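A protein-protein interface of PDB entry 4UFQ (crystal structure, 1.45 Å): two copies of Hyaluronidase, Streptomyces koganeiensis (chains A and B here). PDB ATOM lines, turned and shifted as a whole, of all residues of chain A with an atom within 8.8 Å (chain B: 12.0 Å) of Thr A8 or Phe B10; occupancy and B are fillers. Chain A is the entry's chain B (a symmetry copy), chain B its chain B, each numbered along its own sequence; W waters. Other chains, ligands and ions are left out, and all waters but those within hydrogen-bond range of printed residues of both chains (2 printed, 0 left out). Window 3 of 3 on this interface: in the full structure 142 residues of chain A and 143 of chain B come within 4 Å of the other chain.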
ATOM      1  N   THR A   7     -30.971  -1.690   6.575  1.00  0.00           N
ATOM      2  CA  THR A   7     -31.596  -0.386   6.755  1.00  0.00           C
ATOM      3  C   THR A   7     -31.725  -0.014   8.233  1.00  0.00           C
ATOM      4  O   THR A   7     -31.971  -0.871   9.087  1.00  0.00           O
ATOM      5  CB  THR A   7     -32.992  -0.341   6.110  1.00  0.00           C
ATOM      6  OG1 THR A   7     -32.914  -0.801   4.755  1.00  0.00           O
ATOM      7  CG2 THR A   7     -33.549   1.073   6.133  1.00  0.00           C
ATOM      8  N   THR A   8     -31.560   1.273   8.517  1.00  0.00           N
ATOM      9  CA  THR A   8     -31.640   1.790   9.878  1.00  0.00           C
ATOM     10  C   THR A   8     -32.558   3.010   9.933  1.00  0.00           C
ATOM     11  O   THR A   8     -32.379   3.975   9.193  1.00  0.00           O
ATOM     12  CB  THR A   8     -30.242   2.164  10.408  1.00  0.00           C
ATOM     13  OG1 THR A   8     -29.385   1.017  10.337  1.00  0.00           O
ATOM     14  CG2 THR A   8     -30.316   2.650  11.850  1.00  0.00           C
ATOM     15  N   THR A   9     -33.547   2.954  10.818  1.00  0.00           N
ATOM     16  CA  THR A   9     -34.528   4.022  10.957  1.00  0.00           C
ATOM     17  C   THR A   9     -34.414   4.718  12.314  1.00  0.00           C
ATOM     18  O   THR A   9     -34.688   4.121  13.362  1.00  0.00           O
ATOM     19  CB  THR A   9     -35.963   3.486  10.773  1.00  0.00           C
ATOM     20  OG1 THR A   9     -36.085   2.871   9.484  1.00  0.00           O
ATOM     21  CG2 THR A   9     -36.988   4.606  10.901  1.00  0.00           C
ATOM     22  N   PHE A  10     -34.001   5.980  12.274  1.00  0.00           N
ATOM     23  CA  PHE A  10     -34.015   6.855  13.434  1.00  0.00           C
ATOM     24  C   PHE A  10     -35.352   7.579  13.518  1.00  0.00           C
ATOM     25  O   PHE A  10     -35.741   8.280  12.586  1.00  0.00           O
ATOM     26  CB  PHE A  10     -32.897   7.893  13.332  1.00  0.00           C
ATOM     27  CG  PHE A  10     -31.518   7.306  13.356  1.00  0.00           C
ATOM     28  CD1 PHE A  10     -30.974   6.726  12.223  1.00  0.00           C
ATOM     29  CD2 PHE A  10     -30.761   7.338  14.515  1.00  0.00           C
ATOM     30  CE1 PHE A  10     -29.704   6.188  12.243  1.00  0.00           C
ATOM     31  CE2 PHE A  10     -29.487   6.804  14.541  1.00  0.00           C
ATOM     32  CZ  PHE A  10     -28.959   6.225  13.404  1.00  0.00           C
ATOM     33  N   ASP A  11     -36.044   7.429  14.642  1.00  0.00           N
ATOM     34  CA  ASP A  11     -37.340   8.070  14.832  1.00  0.00           C
ATOM     35  C   ASP A  11     -37.214   9.572  15.104  1.00  0.00           C
ATOM     36  O   ASP A  11     -38.214  10.295  15.073  1.00  0.00           O
ATOM     37  CB  ASP A  11     -38.112   7.399  15.976  1.00  0.00           C
ATOM     38  CG  ASP A  11     -38.686   6.045  15.586  1.00  0.00           C
ATOM     39  OD1 ASP A  11     -38.586   5.661  14.402  1.00  0.00           O
ATOM     40  OD2 ASP A  11     -39.250   5.365  16.469  1.00  0.00           O
ATOM     41  N   VAL A  14     -30.863  13.236  13.678  1.00  0.00           N
ATOM     42  CA  VAL A  14     -29.482  12.801  13.765  1.00  0.00           C
ATOM     43  C   VAL A  14     -28.557  13.995  13.562  1.00  0.00           C
ATOM     44  O   VAL A  14     -28.766  14.818  12.657  1.00  0.00           O
ATOM     45  CB  VAL A  14     -29.163  11.729  12.701  1.00  0.00           C
ATOM     46  CG1 VAL A  14     -27.674  11.394  12.691  1.00  0.00           C
ATOM     47  CG2 VAL A  14     -29.983  10.460  12.952  1.00  0.00           C
ATOM     48  N   ALA A  16     -24.250  14.818  13.367  1.00  0.00           N
ATOM     49  CA  ALA A  16     -22.952  14.179  13.179  1.00  0.00           C
ATOM     50  C   ALA A  16     -21.911  15.202  12.741  1.00  0.00           C
ATOM     51  O   ALA A  16     -22.241  16.348  12.451  1.00  0.00           O
ATOM     52  CB  ALA A  16     -23.057  13.037  12.158  1.00  0.00           C
ATOM     53  N   ARG A  18     -20.139  14.829  10.101  1.00  0.00           N
ATOM     54  CA  ARG A  18     -20.091  14.746   8.646  1.00  0.00           C
ATOM     55  C   ARG A  18     -20.953  13.581   8.180  1.00  0.00           C
ATOM     56  O   ARG A  18     -21.050  12.563   8.871  1.00  0.00           O
ATOM     57  CB  ARG A  18     -18.641  14.535   8.198  1.00  0.00           C
ATOM     58  CG  ARG A  18     -18.455  14.068   6.761  1.00  0.00           C
ATOM     59  CD  ARG A  18     -16.971  13.990   6.427  1.00  0.00           C
ATOM     60  NE  ARG A  18     -16.691  13.179   5.248  1.00  0.00           N
ATOM     61  CZ  ARG A  18     -16.597  13.648   4.005  1.00  0.00           C
ATOM     62  NH1 ARG A  18     -16.769  14.942   3.753  1.00  0.00           N
ATOM     63  NH2 ARG A  18     -16.332  12.816   3.007  1.00  0.00           N
ATOM     64  N   PHE A  19     -21.566  13.731   7.013  1.00  0.00           N
ATOM     65  CA  PHE A  19     -22.317  12.660   6.366  1.00  0.00           C
ATOM     66  C   PHE A  19     -21.724  12.358   5.002  1.00  0.00           C
ATOM     67  O   PHE A  19     -21.520  13.267   4.193  1.00  0.00           O
ATOM     68  CB  PHE A  19     -23.788  13.045   6.194  1.00  0.00           C
ATOM     69  CG  PHE A  19     -24.462  13.432   7.468  1.00  0.00           C
ATOM     70  CD1 PHE A  19     -24.917  12.459   8.346  1.00  0.00           C
ATOM     71  CD2 PHE A  19     -24.627  14.761   7.808  1.00  0.00           C
ATOM     72  CE1 PHE A  19     -25.544  12.809   9.527  1.00  0.00           C
ATOM     73  CE2 PHE A  19     -25.253  15.119   8.987  1.00  0.00           C
ATOM     74  CZ  PHE A  19     -25.706  14.134   9.854  1.00  0.00           C
ATOM     75  N   SER A  20     -21.466  11.088   4.724  1.00  0.00           N
ATOM     76  CA  SER A  20     -20.924  10.707   3.429  1.00  0.00           C
ATOM     77  C   SER A  20     -21.567   9.438   2.905  1.00  0.00           C
ATOM     78  O   SER A  20     -21.933   8.544   3.668  1.00  0.00           O
ATOM     79  CB  SER A  20     -19.405  10.553   3.496  1.00  0.00           C
ATOM     80  OG  SER A  20     -19.043   9.441   4.295  1.00  0.00           O
ATOM     81  N   ALA A  21     -21.717   9.380   1.590  1.00  0.00           N
ATOM     82  CA  ALA A  21     -22.255   8.213   0.919  1.00  0.00           C
ATOM     83  C   ALA A  21     -21.568   8.060  -0.430  1.00  0.00           C
ATOM     84  O   ALA A  21     -21.443   9.024  -1.184  1.00  0.00           O
ATOM     85  CB  ALA A  21     -23.765   8.329   0.751  1.00  0.00           C
ATOM     86  N   ASP A  22     -21.092   6.847  -0.703  1.00  0.00           N
ATOM     87  CA  ASP A  22     -20.545   6.486  -2.009  1.00  0.00           C
ATOM     88  C   ASP A  22     -21.269   5.224  -2.442  1.00  0.00           C
ATOM     89  O   ASP A  22     -20.931   4.128  -2.003  1.00  0.00           O
ATOM     90  CB  ASP A  22     -19.038   6.239  -1.927  1.00  0.00           C
ATOM     91  CG  ASP A  22     -18.392   6.090  -3.297  1.00  0.00           C
ATOM     92  OD1 ASP A  22     -19.127   5.986  -4.301  1.00  0.00           O
ATOM     93  OD2 ASP A  22     -17.146   6.067  -3.366  1.00  0.00           O
ATOM     94  N   THR B   7     -15.736   7.525  14.029  1.00  0.00           N
ATOM     95  CA  THR B   7     -16.418   7.268  12.768  1.00  0.00           C
ATOM     96  C   THR B   7     -17.394   6.095  12.875  1.00  0.00           C
ATOM     97  O   THR B   7     -17.137   5.113  13.579  1.00  0.00           O
ATOM     98  CB  THR B   7     -15.414   6.973  11.639  1.00  0.00           C
ATOM     99  OG1 THR B   7     -14.419   8.002  11.598  1.00  0.00           O
ATOM    100  CG2 THR B   7     -16.123   6.901  10.296  1.00  0.00           C
ATOM    101  N   THR B   8     -18.511   6.211  12.166  1.00  0.00           N
ATOM    102  CA  THR B   8     -19.549   5.186  12.169  1.00  0.00           C
ATOM    103  C   THR B   8     -19.961   4.840  10.738  1.00  0.00           C
ATOM    104  O   THR B   8     -20.321   5.714   9.951  1.00  0.00           O
ATOM    105  CB  THR B   8     -20.781   5.652  12.969  1.00  0.00           C
ATOM    106  OG1 THR B   8     -20.380   5.990  14.304  1.00  0.00           O
ATOM    107  CG2 THR B   8     -21.843   4.562  13.021  1.00  0.00           C
ATOM    108  N   THR B   9     -19.902   3.555  10.411  1.00  0.00           N
ATOM    109  CA  THR B   9     -20.224   3.077   9.073  1.00  0.00           C
ATOM    110  C   THR B   9     -21.478   2.204   9.073  1.00  0.00           C
ATOM    111  O   THR B   9     -21.488   1.102   9.636  1.00  0.00           O
ATOM    112  CB  THR B   9     -19.045   2.286   8.467  1.00  0.00           C
ATOM    113  OG1 THR B   9     -17.879   3.117   8.425  1.00  0.00           O
ATOM    114  CG2 THR B   9     -19.375   1.802   7.061  1.00  0.00           C
ATOM    115  N   PHE B  10     -22.529   2.715   8.442  1.00  0.00           N
ATOM    116  CA  PHE B  10     -23.740   1.956   8.174  1.00  0.00           C
ATOM    117  C   PHE B  10     -23.619   1.249   6.831  1.00  0.00           C
ATOM    118  O   PHE B  10     -23.413   1.895   5.805  1.00  0.00           O
ATOM    119  CB  PHE B  10     -24.953   2.886   8.137  1.00  0.00           C
ATOM    120  CG  PHE B  10     -25.247   3.558   9.444  1.00  0.00           C
ATOM    121  CD1 PHE B  10     -24.517   4.660   9.854  1.00  0.00           C
ATOM    122  CD2 PHE B  10     -26.259   3.088  10.263  1.00  0.00           C
ATOM    123  CE1 PHE B  10     -24.788   5.281  11.057  1.00  0.00           C
ATOM    124  CE2 PHE B  10     -26.537   3.708  11.467  1.00  0.00           C
ATOM    125  CZ  PHE B  10     -25.799   4.803  11.865  1.00  0.00           C
ATOM    126  N   ASP B  11     -23.769  -0.070   6.835  1.00  0.00           N
ATOM    127  CA  ASP B  11     -23.668  -0.853   5.607  1.00  0.00           C
ATOM    128  C   ASP B  11     -24.905  -0.708   4.719  1.00  0.00           C
ATOM    129  O   ASP B  11     -24.891  -1.128   3.559  1.00  0.00           O
ATOM    130  CB  ASP B  11     -23.431  -2.334   5.931  1.00  0.00           C
ATOM    131  CG  ASP B  11     -22.008  -2.618   6.390  1.00  0.00           C
ATOM    132  OD1 ASP B  11     -21.165  -1.696   6.363  1.00  0.00           O
ATOM    133  OD2 ASP B  11     -21.728  -3.772   6.774  1.00  0.00           O
ATOM    134  N   GLY B  12     -25.964  -0.106   5.257  1.00  0.00           N
ATOM    135  CA  GLY B  12     -27.201   0.083   4.520  1.00  0.00           C
ATOM    136  C   GLY B  12     -27.735   1.503   4.596  1.00  0.00           C
ATOM    137  O   GLY B  12     -27.044   2.418   5.051  1.00  0.00           O
ATOM    138  N   PRO B  13     -28.979   1.702   4.142  1.00  0.00           N
ATOM    139  CA  PRO B  13     -29.553   3.051   4.194  1.00  0.00           C
ATOM    140  C   PRO B  13     -29.893   3.504   5.608  1.00  0.00           C
ATOM    141  O   PRO B  13     -30.197   2.689   6.486  1.00  0.00           O
ATOM    142  CB  PRO B  13     -30.835   2.926   3.363  1.00  0.00           C
ATOM    143  CG  PRO B  13     -30.668   1.656   2.561  1.00  0.00           C
ATOM    144  CD  PRO B  13     -29.853   0.758   3.429  1.00  0.00           C
ATOM    145  N   VAL B  14     -29.819   4.814   5.808  1.00  0.00           N
ATOM    146  CA  VAL B  14     -30.250   5.465   7.029  1.00  0.00           C
ATOM    147  C   VAL B  14     -31.422   6.390   6.726  1.00  0.00           C
ATOM    148  O   VAL B  14     -31.404   7.142   5.738  1.00  0.00           O
ATOM    149  CB  VAL B  14     -29.107   6.288   7.660  1.00  0.00           C
ATOM    150  CG1 VAL B  14     -29.610   7.099   8.852  1.00  0.00           C
ATOM    151  CG2 VAL B  14     -27.961   5.370   8.099  1.00  0.00           C
ATOM    152  N   ALA B  15     -32.434   6.329   7.581  1.00  0.00           N
ATOM    153  CA  ALA B  15     -33.568   7.236   7.543  1.00  0.00           C
ATOM    154  C   ALA B  15     -33.665   7.931   8.883  1.00  0.00           C
ATOM    155  O   ALA B  15     -33.421   7.317   9.919  1.00  0.00           O
ATOM    156  CB  ALA B  15     -34.843   6.485   7.251  1.00  0.00           C
ATOM    157  N   ALA B  16     -34.020   9.209   8.865  1.00  0.00           N
ATOM    158  CA  ALA B  16     -34.125   9.991  10.092  1.00  0.00           C
ATOM    159  C   ALA B  16     -35.113  11.138   9.912  1.00  0.00           C
ATOM    160  O   ALA B  16     -35.583  11.393   8.807  1.00  0.00           O
ATOM    161  CB  ALA B  16     -32.747  10.520  10.513  1.00  0.00           C
ATOM    162  N   GLU B  17     -35.435  11.821  11.004  1.00  0.00           N
ATOM    163  CA  GLU B  17     -36.367  12.945  10.957  1.00  0.00           C
ATOM    164  C   GLU B  17     -35.660  14.193  10.435  1.00  0.00           C
ATOM    165  O   GLU B  17     -36.304  15.135   9.972  1.00  0.00           O
ATOM    166  CB  GLU B  17     -36.964  13.219  12.346  1.00  0.00           C
ATOM    167  CG  GLU B  17     -38.107  14.238  12.347  1.00  0.00           C
ATOM    168  CD  GLU B  17     -38.703  14.477  13.728  1.00  0.00           C
ATOM    169  OE1 GLU B  17     -38.073  14.087  14.733  1.00  0.00           O
ATOM    170  OE2 GLU B  17     -39.805  15.065  13.807  1.00  0.00           O
ATOM    171  N   ARG B  18     -34.334  14.186  10.509  1.00  0.00           N
ATOM    172  CA  ARG B  18     -33.530  15.348  10.152  1.00  0.00           C
ATOM    173  C   ARG B  18     -32.054  14.993  10.272  1.00  0.00           C
ATOM    174  O   ARG B  18     -31.672  14.197  11.133  1.00  0.00           O
ATOM    175  CB  ARG B  18     -33.866  16.506  11.097  1.00  0.00           C
ATOM    176  CG  ARG B  18     -32.874  17.662  11.105  1.00  0.00           C
ATOM    177  CD  ARG B  18     -33.380  18.775  12.014  1.00  0.00           C
ATOM    178  NE  ARG B  18     -32.335  19.716  12.404  1.00  0.00           N
ATOM    179  CZ  ARG B  18     -32.045  20.842  11.755  1.00  0.00           C
ATOM    180  NH1 ARG B  18     -32.715  21.187  10.659  1.00  0.00           N
ATOM    181  NH2 ARG B  18     -31.074  21.627  12.203  1.00  0.00           N
ATOM    182  N   PHE B  19     -31.233  15.587   9.414  1.00  0.00           N
ATOM    183  CA  PHE B  19     -29.781  15.458   9.483  1.00  0.00           C
ATOM    184  C   PHE B  19     -29.143  16.824   9.660  1.00  0.00           C
ATOM    185  O   PHE B  19     -29.441  17.756   8.907  1.00  0.00           O
ATOM    186  CB  PHE B  19     -29.225  14.811   8.213  1.00  0.00           C
ATOM    187  CG  PHE B  19     -29.833  13.485   7.896  1.00  0.00           C
ATOM    188  CD1 PHE B  19     -29.404  12.341   8.554  1.00  0.00           C
ATOM    189  CD2 PHE B  19     -30.845  13.373   6.962  1.00  0.00           C
ATOM    190  CE1 PHE B  19     -29.961  11.109   8.266  1.00  0.00           C
ATOM    191  CE2 PHE B  19     -31.406  12.146   6.669  1.00  0.00           C
ATOM    192  CZ  PHE B  19     -30.964  11.009   7.332  1.00  0.00           C
ATOM    193  N   SER B  20     -28.252  16.953  10.631  1.00  0.00           N
ATOM    194  CA  SER B  20     -27.572  18.219  10.852  1.00  0.00           C
ATOM    195  C   SER B  20     -26.102  18.018  11.167  1.00  0.00           C
ATOM    196  O   SER B  20     -25.711  17.032  11.791  1.00  0.00           O
ATOM    197  CB  SER B  20     -28.255  19.021  11.959  1.00  0.00           C
ATOM    198  OG  SER B  20     -28.094  18.389  13.217  1.00  0.00           O
ATOM    199  N   PHE B  29     -20.732  14.726   1.795  1.00  0.00           N
ATOM    200  CA  PHE B  29     -20.196  14.230   0.533  1.00  0.00           C
ATOM    201  C   PHE B  29     -21.127  13.134   0.024  1.00  0.00           C
ATOM    202  O   PHE B  29     -21.199  12.051   0.601  1.00  0.00           O
ATOM    203  CB  PHE B  29     -18.768  13.705   0.709  1.00  0.00           C
ATOM    204  CG  PHE B  29     -18.156  13.178  -0.562  1.00  0.00           C
ATOM    205  CD1 PHE B  29     -17.493  14.026  -1.434  1.00  0.00           C
ATOM    206  CD2 PHE B  29     -18.244  11.833  -0.882  1.00  0.00           C
ATOM    207  CE1 PHE B  29     -16.930  13.539  -2.605  1.00  0.00           C
ATOM    208  CE2 PHE B  29     -17.686  11.342  -2.044  1.00  0.00           C
ATOM    209  CZ  PHE B  29     -17.032  12.198  -2.912  1.00  0.00           C
ATOM    210  N   LEU B  30     -21.857  13.425  -1.046  1.00  0.00           N
ATOM    211  CA  LEU B  30     -22.883  12.520  -1.538  1.00  0.00           C
ATOM    212  C   LEU B  30     -22.559  12.158  -2.967  1.00  0.00           C
ATOM    213  O   LEU B  30     -22.741  12.982  -3.879  1.00  0.00           O
ATOM    214  CB  LEU B  30     -24.262  13.176  -1.438  1.00  0.00           C
ATOM    215  CG  LEU B  30     -24.653  13.619  -0.020  1.00  0.00           C
ATOM    216  CD1 LEU B  30     -25.837  14.559  -0.067  1.00  0.00           C
ATOM    217  CD2 LEU B  30     -24.972  12.419   0.859  1.00  0.00           C
ATOM    218  N   LYS B  31     -22.070  10.938  -3.150  1.00  0.00           N
ATOM    219  CA  LYS B  31     -21.668  10.437  -4.454  1.00  0.00           C
ATOM    220  C   LYS B  31     -22.505   9.226  -4.847  1.00  0.00           C
ATOM    221  O   LYS B  31     -22.624   8.265  -4.093  1.00  0.00           O
ATOM    222  CB  LYS B  31     -20.181  10.084  -4.460  1.00  0.00           C
ATOM    223  CG  LYS B  31     -19.708   9.396  -5.736  1.00  0.00           C
ATOM    224  CD  LYS B  31     -18.225   9.099  -5.679  1.00  0.00           C
ATOM    225  CE  LYS B  31     -17.722   8.508  -6.985  1.00  0.00           C
ATOM    226  NZ  LYS B  31     -16.270   8.170  -6.928  1.00  0.00           N
HETATM  227  O   HOH W   1     -28.760   0.492   7.774  1.00  0.00           O
HETATM  228  O   HOH W   2     -30.196  17.014  13.376  1.00  0.00           O
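The backbone carbonyl oxygen (O) of Pro B13 is in hydrogen-bond range of the backbone NH (N) of Thr A8 (2.8 Å).
The backbone NH of Ala B15 lies within hydrogen-bond range of the backbone carbonyl oxygen of Thr A8 (2.9 Å).
The backbone carbonyl oxygen (O) of Ala B15 is in hydrogen-bond range of the backbone NH (N) of Phe A10 (2.8 Å).
N of Val A14 is in hydrogen-bond range of O of Arg B18 (2.8 Å).
The backbone NH (N) of Ser B20 sits at hydrogen-bond distance from the backbone carbonyl oxygen (O) of Val A14 (3.0 Å).
The backbone carbonyl oxygen of Ser B20 lies within hydrogen-bond range of the backbone NH of Ala A16 (3.1 Å).
The backbone NH (N) of Phe B29 lies within hydrogen-bond range of the backbone carbonyl oxygen (O) of Phe A19 (2.9 Å).
N of Ala A21 is in hydrogen-bond range of O of Phe B29 (2.9 Å).
The backbone carbonyl oxygen of Ala A21 sits at hydrogen-bond distance from the backbone NH of Lys B31, at 2.8 Å.
CD2 of Phe B10 touches OG1 of Thr A8, 3.8 Å away.
Thr A9 touches Ala B15.
CE1 of Phe A10 touches CG1 of Val B14, at 3.5 Å.
CA of Ala B16 touches O of Phe A10, 3.4 Å away.
O of Phe A10 touches N of Glu B17, 3.9 Å away.
CB of Ala B16 touches CG2 of Val A14, 3.7 Å away.
Phe B19 touches Val A14.
Arg A18 touches Phe B29 (NH2 to CB, 3.5 Å).
Phe A19 touches Ser B20 (CE2 to O, 3.4 Å).
Ala A21 touches Leu B30.
Of the printed residues of chain B, Thr A8 touches Phe B10 (3.8 Å), Pro B13 (2.8 Å), Val B14 (3.4 Å) and Ala B15 (2.9 Å).
Thr A7 touches one residue of chain B.
Thr A9 touches just one residue of chain B: Ala B15 (3.6 Å).
Thr B9 touches none of the printed residues of chain A.
No residue of chain A comes within 4 Å of Gly B12.
Of the printed residues of chain A, Ala B16 touches Phe A10 and Val A14.
Of the printed residues of chain A, Arg B18 touches Val A14.
Printed residues of chain A within 4 Å of Phe B29: Arg A18 (3.5 Å), Phe A19 (2.9 Å), Ser A20 (3.1 Å) and Ala A21 (2.9 Å).
Of the printed residues of chain A, Phe B19 touches Val A14 and Phe A19.
Of the printed residues of chain A, Val B14 touches Thr A8 (3.4 Å) and Phe A10 (3.5 Å).
The nearest printed residue of chain B that does not touch Thr A8 is Gly B12 (5.5 Å).
The nearest residue of chain A that does not touch Phe B10 is Thr A7 (6.6 Å).
The nearest printed residue of chain A that does not touch Val B14 is Thr A7 (5.3 Å).
Of the 17 printed residues of chain B, 12 touch a printed residue of chain A.
Hydrophobic or aromatic side chains of chain B within 4 Å of the printed part of chain A: Phe B10, Pro B13, Val B14, Ala B16, Phe B19 and Phe B29.
Of the 12 printed residues of chain A, 12 touch a printed residue of chain B.
Among the printed residues, 26 pairs touch across the chains.
Among the printed residues, no Asp or Glu carboxylate lies within 4 Å of a Lys or Arg side-chain nitrogen of the other chain.
Phe A10 touches its own counterpart, Phe B10.
Phe A10 touches Ala B16, but with the chains exchanged Ala A16 does not touch Phe B10 (8.0 Å).
Ala A16 touches Ser B20, but with the chains exchanged Ser A20 does not touch Ala B16 (12.7 Å).
Phe A19 touches its own counterpart, Phe B19.
Positions printed for both chains: 7, 8, 9, 10, 11, 14, 16, 18, 19 and 20.
Of the 26 pairs that touch across the chains among the printed residues, 2 have their exchanged pair printed and touching as well.
Water W2 bridges OG of Ser B20 and O of Val A14.
Water W1 lies within hydrogen-bond range of OG1 of Thr A8 (2.7 Å), O of Pro B13 (2.9 Å) and N of Thr A7 (3.3 Å).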
